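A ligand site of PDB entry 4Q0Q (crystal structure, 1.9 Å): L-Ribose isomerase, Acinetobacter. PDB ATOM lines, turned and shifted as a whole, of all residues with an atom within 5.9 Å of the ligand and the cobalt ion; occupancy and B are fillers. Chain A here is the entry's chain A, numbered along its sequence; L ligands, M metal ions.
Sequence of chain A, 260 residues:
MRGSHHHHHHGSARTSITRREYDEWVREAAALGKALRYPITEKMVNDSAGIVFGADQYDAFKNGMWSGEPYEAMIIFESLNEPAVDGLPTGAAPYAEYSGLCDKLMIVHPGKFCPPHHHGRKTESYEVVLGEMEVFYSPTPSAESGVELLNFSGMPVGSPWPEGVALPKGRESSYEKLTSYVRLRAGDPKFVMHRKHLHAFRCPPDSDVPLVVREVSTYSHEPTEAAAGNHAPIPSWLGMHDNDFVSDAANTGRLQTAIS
The side-chain carboxylate (OE2) of Glu 222 is in hydrogen-bond range of an oxygen (O4) of the ligand, 2.7 Å away. NZ of Lys 122 sits at hydrogen-bond distance from O3 of the ligand. OE2 of Glu 215 lies within hydrogen-bond range of O3 of the ligand (3.3 Å). SG of Cys 114 sits at hydrogen-bond distance from O5 of the ligand, 3.4 Å away.
The side-chain carboxylate of Glu 124 lies close to the side-chain amino group of Lys 122. OE1 of Glu 124 lies within hydrogen-bond range of OH of Tyr 126 (2.6 Å). A ring nitrogen (ND1) of His 119 lies close to the side-chain amide oxygen of Asn 243 (3.1 Å). The side-chain carboxylate (OE2) of Glu 222 is in salt-bridge range of the guanidinium group (NH1) of Arg 254 (2.8 Å). OE2 of Glu 222 lies within hydrogen-bond range of ND2 of Asn 243. The side-chain carboxylate (OE1) of Glu 222 sits at hydrogen-bond distance from the side-chain hydroxyl (OG) of Ser 220, 2.7 Å away. N of Cys 114 lies within hydrogen-bond range of O of Phe 201, at 2.7 Å. The side-chain sulfur (SG) of Cys 114 lies within hydrogen-bond range of the side-chain sulfur (SD) of Met 74, 3.6 Å away.
Of the 20 residues printed, 4 come within 4 Å of the cobalt ion. Along chain A the residues within 4 Å of the cobalt ion span positions 117 to 199. The nearest printed residue that does not touch the cobalt ion is Lys 122 (4.3 Å).
CD1 of Ile 76 touches C4 of the ligand, 3.6 Å away. CD of Lys 104 touches O3 of the ligand, at 3.9 Å. Met 106 touches the ligand (SD to C1, 3.9 Å). Phe 201 touches the ligand (CE2 to O1, 3.8 Å). Arg 254 touches the ligand. Hydrophobic or aromatic side chains that line the ligand: Ile 76, Met 106, His 117, His 119, His 199 and Phe 201. Within 4 Å of the ligand: Ile 76, Lys 104, Met 106, Cys 114, His 117, His 119, Lys 122, Glu 124, His 199, Phe 201, Glu 215, Glu 222 and Arg 254. The nearest printed residue that does not touch the ligand is Tyr 126 (4.1 Å).
The cobalt ion is bound by OE2 of Glu 124, NE2 of His 199, NE2 of His 119, O2 of the ligand, O1 of the ligand and NE2 of His 117. The cobalt ion has six donor atoms within binding distance.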
ATOM      1  N   ILE A  51     -20.779  11.821  32.306  1.00  0.00           N
ATOM      2  CA  ILE A  51     -19.829  11.772  33.401  1.00  0.00           C
ATOM      3  C   ILE A  51     -20.108  12.804  34.493  1.00  0.00           C
ATOM      4  O   ILE A  51     -20.268  13.988  34.216  1.00  0.00           O
ATOM      5  CB  ILE A  51     -18.404  12.017  32.877  1.00  0.00           C
ATOM      6  CG1 ILE A  51     -18.103  11.027  31.749  1.00  0.00           C
ATOM      7  CG2 ILE A  51     -17.390  11.863  34.009  1.00  0.00           C
ATOM      8  CD1 ILE A  51     -16.848  11.375  30.955  1.00  0.00           C
ATOM      9  N   PHE A  53     -18.323  13.943  37.994  1.00  0.00           N
ATOM     10  CA  PHE A  53     -17.068  13.765  38.735  1.00  0.00           C
ATOM     11  C   PHE A  53     -17.157  13.785  40.263  1.00  0.00           C
ATOM     12  O   PHE A  53     -16.693  14.715  40.921  1.00  0.00           O
ATOM     13  CB  PHE A  53     -16.040  14.807  38.269  1.00  0.00           C
ATOM     14  CG  PHE A  53     -15.720  14.735  36.780  1.00  0.00           C
ATOM     15  CD1 PHE A  53     -16.500  15.415  35.857  1.00  0.00           C
ATOM     16  CD2 PHE A  53     -14.644  13.968  36.325  1.00  0.00           C
ATOM     17  CE1 PHE A  53     -16.205  15.349  34.482  1.00  0.00           C
ATOM     18  CE2 PHE A  53     -14.348  13.888  34.958  1.00  0.00           C
ATOM     19  CZ  PHE A  53     -15.130  14.589  34.039  1.00  0.00           C
ATOM     20  N   MET A  74     -20.101  16.279  32.592  1.00  0.00           N
ATOM     21  CA  MET A  74     -20.024  16.510  31.154  1.00  0.00           C
ATOM     22  C   MET A  74     -20.355  15.250  30.386  1.00  0.00           C
ATOM     23  O   MET A  74     -20.449  14.159  30.952  1.00  0.00           O
ATOM     24  CB  MET A  74     -18.615  16.940  30.772  1.00  0.00           C
ATOM     25  CG  MET A  74     -17.625  15.776  30.742  1.00  0.00           C
ATOM     26  SD  MET A  74     -15.899  16.283  30.699  1.00  0.00           S
ATOM     27  CE  MET A  74     -15.768  16.865  29.002  1.00  0.00           C
ATOM     28  N   ILE A  76     -19.287  12.914  26.957  1.00  0.00           N
ATOM     29  CA  ILE A  76     -18.226  12.643  26.006  1.00  0.00           C
ATOM     30  C   ILE A  76     -18.603  11.469  25.124  1.00  0.00           C
ATOM     31  O   ILE A  76     -18.913  10.384  25.612  1.00  0.00           O
ATOM     32  CB  ILE A  76     -16.887  12.303  26.712  1.00  0.00           C
ATOM     33  CG1 ILE A  76     -16.411  13.497  27.544  1.00  0.00           C
ATOM     34  CG2 ILE A  76     -15.846  11.905  25.675  1.00  0.00           C
ATOM     35  CD1 ILE A  76     -15.138  13.248  28.333  1.00  0.00           C
ATOM     36  N   LYS A 104     -13.138  12.659  20.010  1.00  0.00           N
ATOM     37  CA  LYS A 104     -14.365  12.608  20.778  1.00  0.00           C
ATOM     38  C   LYS A 104     -15.061  13.958  20.800  1.00  0.00           C
ATOM     39  O   LYS A 104     -14.433  15.001  20.611  1.00  0.00           O
ATOM     40  CB  LYS A 104     -14.086  12.152  22.213  1.00  0.00           C
ATOM     41  CG  LYS A 104     -13.411  13.197  23.101  1.00  0.00           C
ATOM     42  CD  LYS A 104     -12.038  12.721  23.585  1.00  0.00           C
ATOM     43  CE  LYS A 104     -11.068  12.568  22.428  1.00  0.00           C
ATOM     44  NZ  LYS A 104      -9.693  12.157  22.862  1.00  0.00           N
ATOM     45  N   MET A 106     -17.221  16.540  23.049  1.00  0.00           N
ATOM     46  CA  MET A 106     -17.483  16.833  24.451  1.00  0.00           C
ATOM     47  C   MET A 106     -18.569  17.882  24.565  1.00  0.00           C
ATOM     48  O   MET A 106     -18.549  18.895  23.865  1.00  0.00           O
ATOM     49  CB  MET A 106     -16.191  17.304  25.135  1.00  0.00           C
ATOM     50  CG  MET A 106     -15.054  16.284  25.019  1.00  0.00           C
ATOM     51  SD  MET A 106     -13.558  16.680  25.984  1.00  0.00           S
ATOM     52  CE  MET A 106     -12.995  18.130  25.118  1.00  0.00           C
ATOM     53  N   CYS A 114     -15.287  20.617  33.145  1.00  0.00           N
ATOM     54  CA  CYS A 114     -14.536  19.400  32.921  1.00  0.00           C
ATOM     55  C   CYS A 114     -13.476  19.856  33.945  1.00  0.00           C
ATOM     56  O   CYS A 114     -12.730  20.813  33.700  1.00  0.00           O
ATOM     57  CB  CYS A 114     -13.897  19.343  31.541  1.00  0.00           C
ATOM     58  SG  CYS A 114     -12.790  17.920  31.378  1.00  0.00           S
ATOM     59  N   HIS A 117      -7.187  18.586  35.929  1.00  0.00           N
ATOM     60  CA  HIS A 117      -6.488  17.319  35.816  1.00  0.00           C
ATOM     61  C   HIS A 117      -5.362  17.471  34.810  1.00  0.00           C
ATOM     62  O   HIS A 117      -5.278  18.465  34.101  1.00  0.00           O
ATOM     63  CB  HIS A 117      -7.432  16.208  35.340  1.00  0.00           C
ATOM     64  CG  HIS A 117      -7.905  16.383  33.924  1.00  0.00           C
ATOM     65  ND1 HIS A 117      -8.868  17.302  33.564  1.00  0.00           N
ATOM     66  CD2 HIS A 117      -7.523  15.774  32.771  1.00  0.00           C
ATOM     67  CE1 HIS A 117      -9.060  17.242  32.256  1.00  0.00           C
ATOM     68  NE2 HIS A 117      -8.263  16.330  31.756  1.00  0.00           N
ATOM     69  N   HIS A 119      -2.473  14.898  32.227  1.00  0.00           N
ATOM     70  CA  HIS A 119      -2.179  13.582  31.695  1.00  0.00           C
ATOM     71  C   HIS A 119      -0.663  13.458  31.597  1.00  0.00           C
ATOM     72  O   HIS A 119       0.026  14.406  31.231  1.00  0.00           O
ATOM     73  CB  HIS A 119      -2.793  13.418  30.308  1.00  0.00           C
ATOM     74  CG  HIS A 119      -4.255  13.711  30.258  1.00  0.00           C
ATOM     75  ND1 HIS A 119      -5.197  12.935  30.888  1.00  0.00           N
ATOM     76  CD2 HIS A 119      -4.943  14.705  29.650  1.00  0.00           C
ATOM     77  CE1 HIS A 119      -6.397  13.438  30.685  1.00  0.00           C
ATOM     78  NE2 HIS A 119      -6.283  14.509  29.931  1.00  0.00           N
ATOM     79  N   LYS A 122      -0.991  11.645  27.481  1.00  0.00           N
ATOM     80  CA  LYS A 122      -1.887  12.240  26.504  1.00  0.00           C
ATOM     81  C   LYS A 122      -1.830  13.746  26.229  1.00  0.00           C
ATOM     82  O   LYS A 122      -1.999  14.564  27.138  1.00  0.00           O
ATOM     83  CB  LYS A 122      -3.335  11.873  26.850  1.00  0.00           C
ATOM     84  CG  LYS A 122      -4.379  12.361  25.844  1.00  0.00           C
ATOM     85  CD  LYS A 122      -5.783  11.858  26.177  1.00  0.00           C
ATOM     86  CE  LYS A 122      -6.591  12.907  26.932  1.00  0.00           C
ATOM     87  NZ  LYS A 122      -7.926  12.376  27.359  1.00  0.00           N
ATOM     88  N   GLU A 124      -3.655  16.742  24.010  1.00  0.00           N
ATOM     89  CA  GLU A 124      -4.928  16.985  23.345  1.00  0.00           C
ATOM     90  C   GLU A 124      -4.994  18.324  22.618  1.00  0.00           C
ATOM     91  O   GLU A 124      -4.127  19.173  22.777  1.00  0.00           O
ATOM     92  CB  GLU A 124      -6.089  16.888  24.360  1.00  0.00           C
ATOM     93  CG  GLU A 124      -5.710  17.210  25.811  1.00  0.00           C
ATOM     94  CD  GLU A 124      -6.874  17.067  26.802  1.00  0.00           C
ATOM     95  OE1 GLU A 124      -7.719  17.973  26.891  1.00  0.00           O
ATOM     96  OE2 GLU A 124      -6.930  16.038  27.515  1.00  0.00           O
ATOM     97  N   TYR A 126      -8.161  21.216  20.953  1.00  0.00           N
ATOM     98  CA  TYR A 126      -9.574  21.564  20.974  1.00  0.00           C
ATOM     99  C   TYR A 126     -10.054  22.333  19.750  1.00  0.00           C
ATOM    100  O   TYR A 126      -9.362  23.190  19.215  1.00  0.00           O
ATOM    101  CB  TYR A 126      -9.904  22.405  22.209  1.00  0.00           C
ATOM    102  CG  TYR A 126      -9.299  21.910  23.494  1.00  0.00           C
ATOM    103  CD1 TYR A 126      -9.440  20.578  23.886  1.00  0.00           C
ATOM    104  CD2 TYR A 126      -8.575  22.772  24.314  1.00  0.00           C
ATOM    105  CE1 TYR A 126      -8.861  20.123  25.066  1.00  0.00           C
ATOM    106  CE2 TYR A 126      -7.992  22.326  25.498  1.00  0.00           C
ATOM    107  CZ  TYR A 126      -8.149  20.995  25.872  1.00  0.00           C
ATOM    108  OH  TYR A 126      -7.580  20.560  27.041  1.00  0.00           O
ATOM    109  N   HIS A 199      -5.132  21.164  33.318  1.00  0.00           N
ATOM    110  CA  HIS A 199      -6.141  21.870  32.554  1.00  0.00           C
ATOM    111  C   HIS A 199      -7.563  21.547  32.991  1.00  0.00           C
ATOM    112  O   HIS A 199      -7.831  20.503  33.589  1.00  0.00           O
ATOM    113  CB  HIS A 199      -5.995  21.619  31.039  1.00  0.00           C
ATOM    114  CG  HIS A 199      -6.151  20.175  30.648  1.00  0.00           C
ATOM    115  ND1 HIS A 199      -5.185  19.225  30.888  1.00  0.00           N
ATOM    116  CD2 HIS A 199      -7.163  19.527  30.018  1.00  0.00           C
ATOM    117  CE1 HIS A 199      -5.590  18.057  30.425  1.00  0.00           C
ATOM    118  NE2 HIS A 199      -6.788  18.216  29.899  1.00  0.00           N
ATOM    119  N   PHE A 201     -11.906  23.179  31.973  1.00  0.00           N
ATOM    120  CA  PHE A 201     -12.682  24.071  31.139  1.00  0.00           C
ATOM    121  C   PHE A 201     -14.166  24.020  31.468  1.00  0.00           C
ATOM    122  O   PHE A 201     -14.648  23.063  32.066  1.00  0.00           O
ATOM    123  CB  PHE A 201     -12.433  23.778  29.640  1.00  0.00           C
ATOM    124  CG  PHE A 201     -12.807  22.383  29.203  1.00  0.00           C
ATOM    125  CD1 PHE A 201     -14.101  22.090  28.779  1.00  0.00           C
ATOM    126  CD2 PHE A 201     -11.841  21.380  29.135  1.00  0.00           C
ATOM    127  CE1 PHE A 201     -14.433  20.822  28.303  1.00  0.00           C
ATOM    128  CE2 PHE A 201     -12.161  20.110  28.653  1.00  0.00           C
ATOM    129  CZ  PHE A 201     -13.465  19.828  28.238  1.00  0.00           C
ATOM    130  N   GLU A 215     -12.422  17.073  20.563  1.00  0.00           N
ATOM    131  CA  GLU A 215     -11.064  16.900  21.014  1.00  0.00           C
ATOM    132  C   GLU A 215     -10.362  15.891  20.116  1.00  0.00           C
ATOM    133  O   GLU A 215     -10.914  14.828  19.825  1.00  0.00           O
ATOM    134  CB  GLU A 215     -11.018  16.399  22.452  1.00  0.00           C
ATOM    135  CG  GLU A 215      -9.608  16.085  22.926  1.00  0.00           C
ATOM    136  CD  GLU A 215      -9.579  15.518  24.317  1.00  0.00           C
ATOM    137  OE1 GLU A 215      -9.882  16.278  25.261  1.00  0.00           O
ATOM    138  OE2 GLU A 215      -9.241  14.323  24.471  1.00  0.00           O
ATOM    139  N   SER A 220      -6.234   7.633  24.731  1.00  0.00           N
ATOM    140  CA  SER A 220      -6.800   7.871  26.054  1.00  0.00           C
ATOM    141  C   SER A 220      -6.836   6.583  26.882  1.00  0.00           C
ATOM    142  O   SER A 220      -7.605   5.659  26.603  1.00  0.00           O
ATOM    143  CB  SER A 220      -8.211   8.452  25.897  1.00  0.00           C
ATOM    144  OG  SER A 220      -8.748   8.797  27.159  1.00  0.00           O
ATOM    145  N   GLU A 222      -8.122   5.084  29.754  1.00  0.00           N
ATOM    146  CA  GLU A 222      -9.151   5.257  30.774  1.00  0.00           C
ATOM    147  C   GLU A 222      -9.962   3.980  31.022  1.00  0.00           C
ATOM    148  O   GLU A 222     -10.822   3.620  30.230  1.00  0.00           O
ATOM    149  CB  GLU A 222     -10.116   6.370  30.360  1.00  0.00           C
ATOM    150  CG  GLU A 222      -9.458   7.728  30.128  1.00  0.00           C
ATOM    151  CD  GLU A 222     -10.452   8.786  29.652  1.00  0.00           C
ATOM    152  OE1 GLU A 222     -11.010   8.624  28.542  1.00  0.00           O
ATOM    153  OE2 GLU A 222     -10.661   9.773  30.380  1.00  0.00           O
ATOM    154  N   ASN A 243      -5.206   9.495  33.716  1.00  0.00           N
ATOM    155  CA  ASN A 243      -5.901  10.691  34.187  1.00  0.00           C
ATOM    156  C   ASN A 243      -5.523  10.936  35.630  1.00  0.00           C
ATOM    157  O   ASN A 243      -5.541  10.018  36.457  1.00  0.00           O
ATOM    158  CB  ASN A 243      -7.419  10.539  34.101  1.00  0.00           C
ATOM    159  CG  ASN A 243      -7.905  10.377  32.685  1.00  0.00           C
ATOM    160  OD1 ASN A 243      -7.229  10.767  31.730  1.00  0.00           O
ATOM    161  ND2 ASN A 243      -9.107   9.825  32.533  1.00  0.00           N
ATOM    162  N   PHE A 245      -6.755  13.628  38.289  1.00  0.00           N
ATOM    163  CA  PHE A 245      -7.572  14.761  38.687  1.00  0.00           C
ATOM    164  C   PHE A 245      -7.096  15.322  40.028  1.00  0.00           C
ATOM    165  O   PHE A 245      -6.776  14.563  40.953  1.00  0.00           O
ATOM    166  CB  PHE A 245      -9.037  14.322  38.780  1.00  0.00           C
ATOM    167  CG  PHE A 245      -9.672  14.062  37.451  1.00  0.00           C
ATOM    168  CD1 PHE A 245     -10.307  15.099  36.753  1.00  0.00           C
ATOM    169  CD2 PHE A 245      -9.595  12.805  36.853  1.00  0.00           C
ATOM    170  CE1 PHE A 245     -10.854  14.873  35.485  1.00  0.00           C
ATOM    171  CE2 PHE A 245     -10.137  12.573  35.597  1.00  0.00           C
ATOM    172  CZ  PHE A 245     -10.772  13.609  34.899  1.00  0.00           C
ATOM    173  N   ARG A 254     -14.998   9.715  37.515  1.00  0.00           N
ATOM    174  CA  ARG A 254     -14.746   9.643  36.084  1.00  0.00           C
ATOM    175  C   ARG A 254     -14.995   8.238  35.511  1.00  0.00           C
ATOM    176  O   ARG A 254     -15.548   8.100  34.421  1.00  0.00           O
ATOM    177  CB  ARG A 254     -13.297  10.054  35.795  1.00  0.00           C
ATOM    178  CG  ARG A 254     -13.016  10.532  34.358  1.00  0.00           C
ATOM    179  CD  ARG A 254     -13.386   9.493  33.309  1.00  0.00           C
ATOM    180  NE  ARG A 254     -13.100   9.938  31.945  1.00  0.00           N
ATOM    181  CZ  ARG A 254     -13.637   9.408  30.855  1.00  0.00           C
ATOM    182  NH1 ARG A 254     -13.321   9.865  29.656  1.00  0.00           N
ATOM    183  NH2 ARG A 254     -14.519   8.415  30.971  1.00  0.00           N
HETATM  184  C1  LIG L   1     -10.397  16.613  28.221  1.00  0.00           C
HETATM  185  O1  LIG L   1      -9.437  17.445  28.861  1.00  0.00           O
HETATM  186  C2  LIG L   1     -10.422  15.233  28.849  1.00  0.00           C
HETATM  187  O2  LIG L   1      -9.123  14.654  28.796  1.00  0.00           O
HETATM  188  C3  LIG L   1     -11.431  14.269  28.266  1.00  0.00           C
HETATM  189  O3  LIG L   1     -10.835  13.483  27.250  1.00  0.00           O
HETATM  190  C4  LIG L   1     -11.773  13.386  29.470  1.00  0.00           C
HETATM  191  O4  LIG L   1     -10.777  12.377  29.608  1.00  0.00           O
HETATM  192  C5  LIG L   1     -11.662  14.347  30.649  1.00  0.00           C
HETATM  193  O5  LIG L   1     -10.767  15.391  30.234  1.00  0.00           O
HETATM  194 CO    CO M   1      -7.602  16.217  29.533  1.00  0.00          CO
